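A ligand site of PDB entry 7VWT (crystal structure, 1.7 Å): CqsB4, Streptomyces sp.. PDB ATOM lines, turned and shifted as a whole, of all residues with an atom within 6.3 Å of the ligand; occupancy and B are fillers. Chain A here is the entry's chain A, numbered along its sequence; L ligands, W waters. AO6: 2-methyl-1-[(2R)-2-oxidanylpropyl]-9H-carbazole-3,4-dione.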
ATOM      1  N   ARG A  36      -0.709   0.574 -14.503  1.00  0.00           N
ATOM      2  CA  ARG A  36      -0.633   1.941 -14.011  1.00  0.00           C
ATOM      3  C   ARG A  36      -0.303   1.997 -12.520  1.00  0.00           C
ATOM      4  O   ARG A  36       0.282   2.965 -12.061  1.00  0.00           O
ATOM      5  CB  ARG A  36      -1.942   2.697 -14.264  1.00  0.00           C
ATOM      6  CG  ARG A  36      -2.287   2.850 -15.762  1.00  0.00           C
ATOM      7  CD  ARG A  36      -3.762   3.253 -15.998  1.00  0.00           C
ATOM      8  NE  ARG A  36      -4.737   2.165 -15.793  1.00  0.00           N
ATOM      9  CZ  ARG A  36      -6.055   2.284 -15.986  1.00  0.00           C
ATOM     10  NH1 ARG A  36      -6.869   1.261 -15.772  1.00  0.00           N
ATOM     11  NH2 ARG A  36      -6.567   3.438 -16.411  1.00  0.00           N
ATOM     12  N   PHE A  51      -1.317   9.710  -4.508  1.00  0.00           N
ATOM     13  CA  PHE A  51      -1.220   9.240  -5.881  1.00  0.00           C
ATOM     14  C   PHE A  51      -2.146   8.052  -6.082  1.00  0.00           C
ATOM     15  O   PHE A  51      -2.935   8.018  -7.037  1.00  0.00           O
ATOM     16  CB  PHE A  51       0.228   8.842  -6.184  1.00  0.00           C
ATOM     17  CG  PHE A  51       0.454   8.280  -7.567  1.00  0.00           C
ATOM     18  CD1 PHE A  51       0.825   9.106  -8.626  1.00  0.00           C
ATOM     19  CD2 PHE A  51       0.280   6.907  -7.815  1.00  0.00           C
ATOM     20  CE1 PHE A  51       1.081   8.571  -9.922  1.00  0.00           C
ATOM     21  CE2 PHE A  51       0.525   6.369  -9.102  1.00  0.00           C
ATOM     22  CZ  PHE A  51       0.920   7.206 -10.150  1.00  0.00           C
ATOM     23  N   PHE A  54      -5.923   9.094  -5.784  1.00  0.00           N
ATOM     24  CA  PHE A  54      -6.447   9.851  -6.914  1.00  0.00           C
ATOM     25  C   PHE A  54      -6.588   8.971  -8.154  1.00  0.00           C
ATOM     26  O   PHE A  54      -7.656   8.907  -8.767  1.00  0.00           O
ATOM     27  CB  PHE A  54      -5.588  11.093  -7.218  1.00  0.00           C
ATOM     28  CG  PHE A  54      -6.307  12.099  -8.098  1.00  0.00           C
ATOM     29  CD1 PHE A  54      -7.077  13.103  -7.528  1.00  0.00           C
ATOM     30  CD2 PHE A  54      -6.275  11.983  -9.475  1.00  0.00           C
ATOM     31  CE1 PHE A  54      -7.769  14.018  -8.350  1.00  0.00           C
ATOM     32  CE2 PHE A  54      -6.966  12.865 -10.281  1.00  0.00           C
ATOM     33  CZ  PHE A  54      -7.701  13.883  -9.708  1.00  0.00           C
ATOM     34  N   PHE A  55      -5.511   8.231  -8.511  1.00  0.00           N
ATOM     35  CA  PHE A  55      -5.632   7.347  -9.663  1.00  0.00           C
ATOM     36  C   PHE A  55      -6.728   6.336  -9.444  1.00  0.00           C
ATOM     37  O   PHE A  55      -7.482   6.008 -10.380  1.00  0.00           O
ATOM     38  CB  PHE A  55      -4.326   6.625  -9.920  1.00  0.00           C
ATOM     39  CG  PHE A  55      -3.559   7.182 -11.055  1.00  0.00           C
ATOM     40  CD1 PHE A  55      -3.908   6.864 -12.360  1.00  0.00           C
ATOM     41  CD2 PHE A  55      -2.500   8.033 -10.834  1.00  0.00           C
ATOM     42  CE1 PHE A  55      -3.191   7.386 -13.426  1.00  0.00           C
ATOM     43  CE2 PHE A  55      -1.776   8.553 -11.893  1.00  0.00           C
ATOM     44  CZ  PHE A  55      -2.142   8.225 -13.188  1.00  0.00           C
ATOM     45  N   VAL A  58     -10.037   7.896 -10.460  1.00  0.00           N
ATOM     46  CA  VAL A  58     -10.264   8.006 -11.907  1.00  0.00           C
ATOM     47  C   VAL A  58     -10.449   6.624 -12.552  1.00  0.00           C
ATOM     48  O   VAL A  58     -11.363   6.418 -13.354  1.00  0.00           O
ATOM     49  CB  VAL A  58      -9.130   8.809 -12.542  1.00  0.00           C
ATOM     50  CG1 VAL A  58      -9.318   8.863 -14.049  1.00  0.00           C
ATOM     51  CG2 VAL A  58      -9.160  10.193 -11.936  1.00  0.00           C
ATOM     52  N   VAL A 155     -14.405  15.128 -18.453  1.00  0.00           N
ATOM     53  CA  VAL A 155     -13.963  13.760 -18.178  1.00  0.00           C
ATOM     54  C   VAL A 155     -12.445  13.668 -18.069  1.00  0.00           C
ATOM     55  O   VAL A 155     -11.929  13.003 -17.179  1.00  0.00           O
ATOM     56  CB  VAL A 155     -14.508  12.794 -19.242  1.00  0.00           C
ATOM     57  CG1 VAL A 155     -13.799  11.407 -19.144  1.00  0.00           C
ATOM     58  CG2 VAL A 155     -16.045  12.685 -19.121  1.00  0.00           C
ATOM     59  N   THR A 156     -11.725  14.362 -18.944  1.00  0.00           N
ATOM     60  CA  THR A 156     -10.283  14.202 -19.107  1.00  0.00           C
ATOM     61  C   THR A 156      -9.510  15.220 -18.287  1.00  0.00           C
ATOM     62  O   THR A 156      -8.626  14.858 -17.508  1.00  0.00           O
ATOM     63  CB  THR A 156      -9.877  14.335 -20.590  1.00  0.00           C
ATOM     64  OG1 THR A 156     -10.611  13.407 -21.389  1.00  0.00           O
ATOM     65  CG2 THR A 156      -8.371  14.088 -20.828  1.00  0.00           C
ATOM     66  N   LEU A 158     -10.449  17.879 -16.139  1.00  0.00           N
ATOM     67  CA  LEU A 158     -10.754  18.315 -14.782  1.00  0.00           C
ATOM     68  C   LEU A 158      -9.937  17.523 -13.774  1.00  0.00           C
ATOM     69  O   LEU A 158      -9.164  18.129 -13.008  1.00  0.00           O
ATOM     70  CB  LEU A 158     -12.253  18.222 -14.542  1.00  0.00           C
ATOM     71  CG  LEU A 158     -12.726  18.752 -13.181  1.00  0.00           C
ATOM     72  CD1 LEU A 158     -12.391  20.233 -13.043  1.00  0.00           C
ATOM     73  CD2 LEU A 158     -14.241  18.503 -12.961  1.00  0.00           C
ATOM     74  N   PRO A 159     -10.016  16.182 -13.734  1.00  0.00           N
ATOM     75  CA  PRO A 159      -9.129  15.420 -12.852  1.00  0.00           C
ATOM     76  C   PRO A 159      -7.662  15.606 -13.157  1.00  0.00           C
ATOM     77  O   PRO A 159      -6.850  15.635 -12.209  1.00  0.00           O
ATOM     78  CB  PRO A 159      -9.589  13.964 -13.080  1.00  0.00           C
ATOM     79  CG  PRO A 159     -10.154  13.984 -14.482  1.00  0.00           C
ATOM     80  CD  PRO A 159     -10.885  15.318 -14.553  1.00  0.00           C
ATOM     81  N   ALA A 160      -7.273  15.753 -14.438  1.00  0.00           N
ATOM     82  CA  ALA A 160      -5.865  15.977 -14.752  1.00  0.00           C
ATOM     83  C   ALA A 160      -5.316  17.193 -14.010  1.00  0.00           C
ATOM     84  O   ALA A 160      -4.240  17.102 -13.395  1.00  0.00           O
ATOM     85  CB  ALA A 160      -5.650  16.097 -16.270  1.00  0.00           C
ATOM     86  N   ILE A 161      -6.025  18.337 -14.035  1.00  0.00           N
ATOM     87  CA  ILE A 161      -5.463  19.558 -13.433  1.00  0.00           C
ATOM     88  C   ILE A 161      -5.465  19.480 -11.901  1.00  0.00           C
ATOM     89  O   ILE A 161      -4.673  20.160 -11.232  1.00  0.00           O
ATOM     90  CB  ILE A 161      -6.187  20.847 -13.900  1.00  0.00           C
ATOM     91  CG1 ILE A 161      -7.636  20.919 -13.417  1.00  0.00           C
ATOM     92  CG2 ILE A 161      -6.106  21.007 -15.432  1.00  0.00           C
ATOM     93  CD1 ILE A 161      -8.297  22.308 -13.670  1.00  0.00           C
ATOM     94  N   ILE A 163      -4.801  16.362 -10.192  1.00  0.00           N
ATOM     95  CA  ILE A 163      -3.605  15.588  -9.831  1.00  0.00           C
ATOM     96  C   ILE A 163      -2.351  16.379 -10.146  1.00  0.00           C
ATOM     97  O   ILE A 163      -1.307  16.205  -9.503  1.00  0.00           O
ATOM     98  CB  ILE A 163      -3.576  14.211 -10.512  1.00  0.00           C
ATOM     99  CG1 ILE A 163      -2.631  13.296  -9.732  1.00  0.00           C
ATOM    100  CG2 ILE A 163      -3.256  14.289 -12.008  1.00  0.00           C
ATOM    101  CD1 ILE A 163      -2.608  11.858 -10.231  1.00  0.00           C
ATOM    102  N   PHE A 167       1.160  16.579  -8.023  1.00  0.00           N
ATOM    103  CA  PHE A 167       2.513  16.398  -8.514  1.00  0.00           C
ATOM    104  C   PHE A 167       3.426  17.514  -7.997  1.00  0.00           C
ATOM    105  O   PHE A 167       4.643  17.405  -8.138  1.00  0.00           O
ATOM    106  CB  PHE A 167       2.533  16.388 -10.047  1.00  0.00           C
ATOM    107  CG  PHE A 167       1.942  15.168 -10.678  1.00  0.00           C
ATOM    108  CD1 PHE A 167       1.844  13.972  -9.980  1.00  0.00           C
ATOM    109  CD2 PHE A 167       1.477  15.217 -11.981  1.00  0.00           C
ATOM    110  CE1 PHE A 167       1.287  12.834 -10.588  1.00  0.00           C
ATOM    111  CE2 PHE A 167       0.936  14.090 -12.599  1.00  0.00           C
ATOM    112  CZ  PHE A 167       0.861  12.903 -11.904  1.00  0.00           C
ATOM    113  N   ILE A 182      -2.052  15.646 -21.282  1.00  0.00           N
ATOM    114  CA  ILE A 182      -3.161  14.703 -21.072  1.00  0.00           C
ATOM    115  C   ILE A 182      -4.148  14.766 -22.234  1.00  0.00           C
ATOM    116  O   ILE A 182      -4.775  13.742 -22.584  1.00  0.00           O
ATOM    117  CB  ILE A 182      -3.861  14.966 -19.714  1.00  0.00           C
ATOM    118  CG1 ILE A 182      -2.910  14.755 -18.501  1.00  0.00           C
ATOM    119  CG2 ILE A 182      -5.063  14.030 -19.482  1.00  0.00           C
ATOM    120  CD1 ILE A 182      -2.055  13.459 -18.478  1.00  0.00           C
ATOM    121  N   PHE A 185      -2.592  12.362 -24.676  1.00  0.00           N
ATOM    122  CA  PHE A 185      -2.902  10.994 -24.253  1.00  0.00           C
ATOM    123  C   PHE A 185      -4.326  10.602 -24.590  1.00  0.00           C
ATOM    124  O   PHE A 185      -4.599   9.447 -24.982  1.00  0.00           O
ATOM    125  CB  PHE A 185      -2.712  10.842 -22.737  1.00  0.00           C
ATOM    126  CG  PHE A 185      -1.286  10.985 -22.252  1.00  0.00           C
ATOM    127  CD1 PHE A 185      -0.223  11.244 -23.118  1.00  0.00           C
ATOM    128  CD2 PHE A 185      -1.032  10.858 -20.897  1.00  0.00           C
ATOM    129  CE1 PHE A 185       1.071  11.372 -22.613  1.00  0.00           C
ATOM    130  CE2 PHE A 185       0.245  11.013 -20.382  1.00  0.00           C
ATOM    131  CZ  PHE A 185       1.308  11.259 -21.253  1.00  0.00           C
ATOM    132  N   GLN A 186      -5.271  11.507 -24.341  1.00  0.00           N
ATOM    133  CA  GLN A 186      -6.673  11.127 -24.522  1.00  0.00           C
ATOM    134  C   GLN A 186      -7.012  10.985 -25.992  1.00  0.00           C
ATOM    135  O   GLN A 186      -7.776  10.106 -26.388  1.00  0.00           O
ATOM    136  CB  GLN A 186      -7.579  12.165 -23.847  1.00  0.00           C
ATOM    137  CG  GLN A 186      -9.013  11.969 -24.028  1.00  0.00           C
ATOM    138  CD  GLN A 186      -9.478  10.752 -23.244  1.00  0.00           C
ATOM    139  OE1 GLN A 186      -9.788  10.872 -22.065  1.00  0.00           O
ATOM    140  NE2 GLN A 186      -9.527   9.590 -23.880  1.00  0.00           N
ATOM    141  N   LEU A 187      -6.474  11.878 -26.824  1.00  0.00           N
ATOM    142  CA  LEU A 187      -6.668  11.742 -28.263  1.00  0.00           C
ATOM    143  C   LEU A 187      -6.008  10.485 -28.806  1.00  0.00           C
ATOM    144  O   LEU A 187      -6.498   9.884 -29.756  1.00  0.00           O
ATOM    145  CB  LEU A 187      -6.091  12.965 -28.964  1.00  0.00           C
ATOM    146  CG  LEU A 187      -6.838  14.260 -28.603  1.00  0.00           C
ATOM    147  CD1 LEU A 187      -6.156  15.441 -29.281  1.00  0.00           C
ATOM    148  CD2 LEU A 187      -8.332  14.176 -28.991  1.00  0.00           C
ATOM    149  N   ASP A 189      -5.764   7.756 -27.203  1.00  0.00           N
ATOM    150  CA  ASP A 189      -6.694   6.689 -26.844  1.00  0.00           C
ATOM    151  C   ASP A 189      -7.830   6.598 -27.842  1.00  0.00           C
ATOM    152  O   ASP A 189      -8.198   5.499 -28.275  1.00  0.00           O
ATOM    153  CB  ASP A 189      -7.213   6.901 -25.435  1.00  0.00           C
ATOM    154  CG  ASP A 189      -6.568   5.974 -24.449  1.00  0.00           C
ATOM    155  OD1 ASP A 189      -5.487   5.415 -24.769  1.00  0.00           O
ATOM    156  OD2 ASP A 189      -7.152   5.773 -23.368  1.00  0.00           O
ATOM    157  N   TRP A 254       6.231  19.657 -19.622  1.00  0.00           N
ATOM    158  CA  TRP A 254       5.537  19.458 -18.350  1.00  0.00           C
ATOM    159  C   TRP A 254       6.422  18.877 -17.257  1.00  0.00           C
ATOM    160  O   TRP A 254       6.387  19.391 -16.128  1.00  0.00           O
ATOM    161  CB  TRP A 254       4.316  18.565 -18.586  1.00  0.00           C
ATOM    162  CG  TRP A 254       3.373  18.468 -17.442  1.00  0.00           C
ATOM    163  CD1 TRP A 254       3.261  19.324 -16.401  1.00  0.00           C
ATOM    164  CD2 TRP A 254       2.369  17.453 -17.232  1.00  0.00           C
ATOM    165  NE1 TRP A 254       2.292  18.935 -15.542  1.00  0.00           N
ATOM    166  CE2 TRP A 254       1.710  17.773 -16.020  1.00  0.00           C
ATOM    167  CE3 TRP A 254       1.982  16.308 -17.937  1.00  0.00           C
ATOM    168  CZ2 TRP A 254       0.681  17.025 -15.517  1.00  0.00           C
ATOM    169  CZ3 TRP A 254       0.959  15.554 -17.440  1.00  0.00           C
ATOM    170  CH2 TRP A 254       0.298  15.922 -16.239  1.00  0.00           C
ATOM    171  N   PHE A 265       8.056   9.776 -13.172  1.00  0.00           N
ATOM    172  CA  PHE A 265       6.745   9.230 -13.511  1.00  0.00           C
ATOM    173  C   PHE A 265       6.212   9.838 -14.809  1.00  0.00           C
ATOM    174  O   PHE A 265       5.812   9.109 -15.722  1.00  0.00           O
ATOM    175  CB  PHE A 265       5.726   9.465 -12.394  1.00  0.00           C
ATOM    176  CG  PHE A 265       4.323   9.098 -12.818  1.00  0.00           C
ATOM    177  CD1 PHE A 265       3.934   7.771 -12.882  1.00  0.00           C
ATOM    178  CD2 PHE A 265       3.422  10.079 -13.221  1.00  0.00           C
ATOM    179  CE1 PHE A 265       2.653   7.413 -13.282  1.00  0.00           C
ATOM    180  CE2 PHE A 265       2.146   9.743 -13.619  1.00  0.00           C
ATOM    181  CZ  PHE A 265       1.752   8.401 -13.658  1.00  0.00           C
ATOM    182  N   MET A 266       6.174  11.168 -14.917  1.00  0.00           N
ATOM    183  CA  MET A 266       5.553  11.728 -16.106  1.00  0.00           C
ATOM    184  C   MET A 266       6.462  11.604 -17.327  1.00  0.00           C
ATOM    185  O   MET A 266       5.971  11.472 -18.441  1.00  0.00           O
ATOM    186  CB  MET A 266       5.117  13.170 -15.882  1.00  0.00           C
ATOM    187  CG  MET A 266       4.266  13.738 -17.031  1.00  0.00           C
ATOM    188  SD  MET A 266       2.945  12.668 -17.644  1.00  0.00           S
ATOM    189  CE  MET A 266       1.931  12.555 -16.174  1.00  0.00           C
ATOM    190  N   ASP A 269       5.585   8.103 -18.458  1.00  0.00           N
ATOM    191  CA  ASP A 269       4.230   8.038 -19.028  1.00  0.00           C
ATOM    192  C   ASP A 269       4.197   8.646 -20.432  1.00  0.00           C
ATOM    193  O   ASP A 269       3.557   8.124 -21.331  1.00  0.00           O
ATOM    194  CB  ASP A 269       3.273   8.752 -18.107  1.00  0.00           C
ATOM    195  CG  ASP A 269       1.847   8.354 -18.326  1.00  0.00           C
ATOM    196  OD1 ASP A 269       1.590   7.367 -19.036  1.00  0.00           O
ATOM    197  OD2 ASP A 269       0.989   9.053 -17.776  1.00  0.00           O
ATOM    198  N   HIS A 273       3.261   6.608 -23.964  1.00  0.00           N
ATOM    199  CA  HIS A 273       2.272   7.039 -24.953  1.00  0.00           C
ATOM    200  C   HIS A 273       2.933   7.399 -26.270  1.00  0.00           C
ATOM    201  O   HIS A 273       2.365   7.174 -27.323  1.00  0.00           O
ATOM    202  CB  HIS A 273       1.451   8.227 -24.434  1.00  0.00           C
ATOM    203  CG  HIS A 273       0.482   7.866 -23.371  1.00  0.00           C
ATOM    204  ND1 HIS A 273       0.816   7.805 -22.033  1.00  0.00           N
ATOM    205  CD2 HIS A 273      -0.812   7.453 -23.437  1.00  0.00           C
ATOM    206  CE1 HIS A 273      -0.214   7.367 -21.335  1.00  0.00           C
ATOM    207  NE2 HIS A 273      -1.216   7.163 -22.171  1.00  0.00           N
HETATM  208  CAS AO6 L   1      -5.210  10.905 -13.169  1.00  0.00           C
HETATM  209  CAR AO6 L   1      -5.715  11.526 -14.485  1.00  0.00           C
HETATM  210  OAT AO6 L   1      -6.811  12.323 -14.148  1.00  0.00           O
HETATM  211  CAQ AO6 L   1      -4.670  12.356 -15.212  1.00  0.00           C
HETATM  212  CAJ AO6 L   1      -3.814  11.387 -15.996  1.00  0.00           C
HETATM  213  CAH AO6 L   1      -4.365  10.753 -17.285  1.00  0.00           C
HETATM  214  NAG AO6 L   1      -5.581  11.001 -17.861  1.00  0.00           N
HETATM  215  CAD AO6 L   1      -5.605  10.243 -18.988  1.00  0.00           C
HETATM  216  CAC AO6 L   1      -6.707  10.085 -20.058  1.00  0.00           C
HETATM  217  CAB AO6 L   1      -6.457   9.161 -21.188  1.00  0.00           C
HETATM  218  CAA AO6 L   1      -5.193   8.390 -21.309  1.00  0.00           C
HETATM  219  CAF AO6 L   1      -4.122   8.555 -20.291  1.00  0.00           C
HETATM  220  CAE AO6 L   1      -4.383   9.538 -19.109  1.00  0.00           C
HETATM  221  CAI AO6 L   1      -3.590   9.837 -18.029  1.00  0.00           C
HETATM  222  CAM AO6 L   1      -2.143   9.379 -17.604  1.00  0.00           C
HETATM  223  OAN AO6 L   1      -1.488   8.572 -18.248  1.00  0.00           O
HETATM  224  CAL AO6 L   1      -1.621   9.986 -16.352  1.00  0.00           C
HETATM  225  OAO AO6 L   1      -0.530   9.723 -15.929  1.00  0.00           O
HETATM  226  CAK AO6 L   1      -2.449  10.968 -15.586  1.00  0.00           C
HETATM  227  CAP AO6 L   1      -1.904  11.577 -14.312  1.00  0.00           C
HETATM  228  O   HOH W   1      -7.926  12.299 -16.815  1.00  0.00           O
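An oxygen (OAO) of the ligand lies close to the side-chain carboxylate of Asp 269. The backbone NH (N) of Ala 160 sits at hydrogen-bond distance from an oxygen (OAT) of the ligand, at 3.5 Å.
OG1 of Thr 156 sits at hydrogen-bond distance from OE1 of Gln 186, at 2.7 Å. The backbone carbonyl oxygen (O) of Asp 269 lies within hydrogen-bond range of a ring nitrogen (ND1) of His 273, 2.8 Å away.
Residues that only touch the ligand: Phe 54 (3.9 Å), Phe 55 (3.5 Å), Val 58 (3.9 Å), Pro 159 (3.4 Å), Ile 163 (3.8 Å), Phe 167 (3.9 Å), Ile 182 (3.5 Å), Phe 185 (3.5 Å), Gln 186 (3.8 Å), Asp 189 (3.9 Å), Phe 265 (3.5 Å), Met 266 (3.8 Å) and His 273 (3.6 Å). Hydrophobic or aromatic side chains that line the ligand: Phe 54, Phe 55, Val 58, Pro 159, Ile 163, Phe 167, Ile 182, Phe 185, Phe 265, Met 266 and His 273.
Water W1 lies within hydrogen-bond range of O of Thr 156 and NAG of the ligand.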
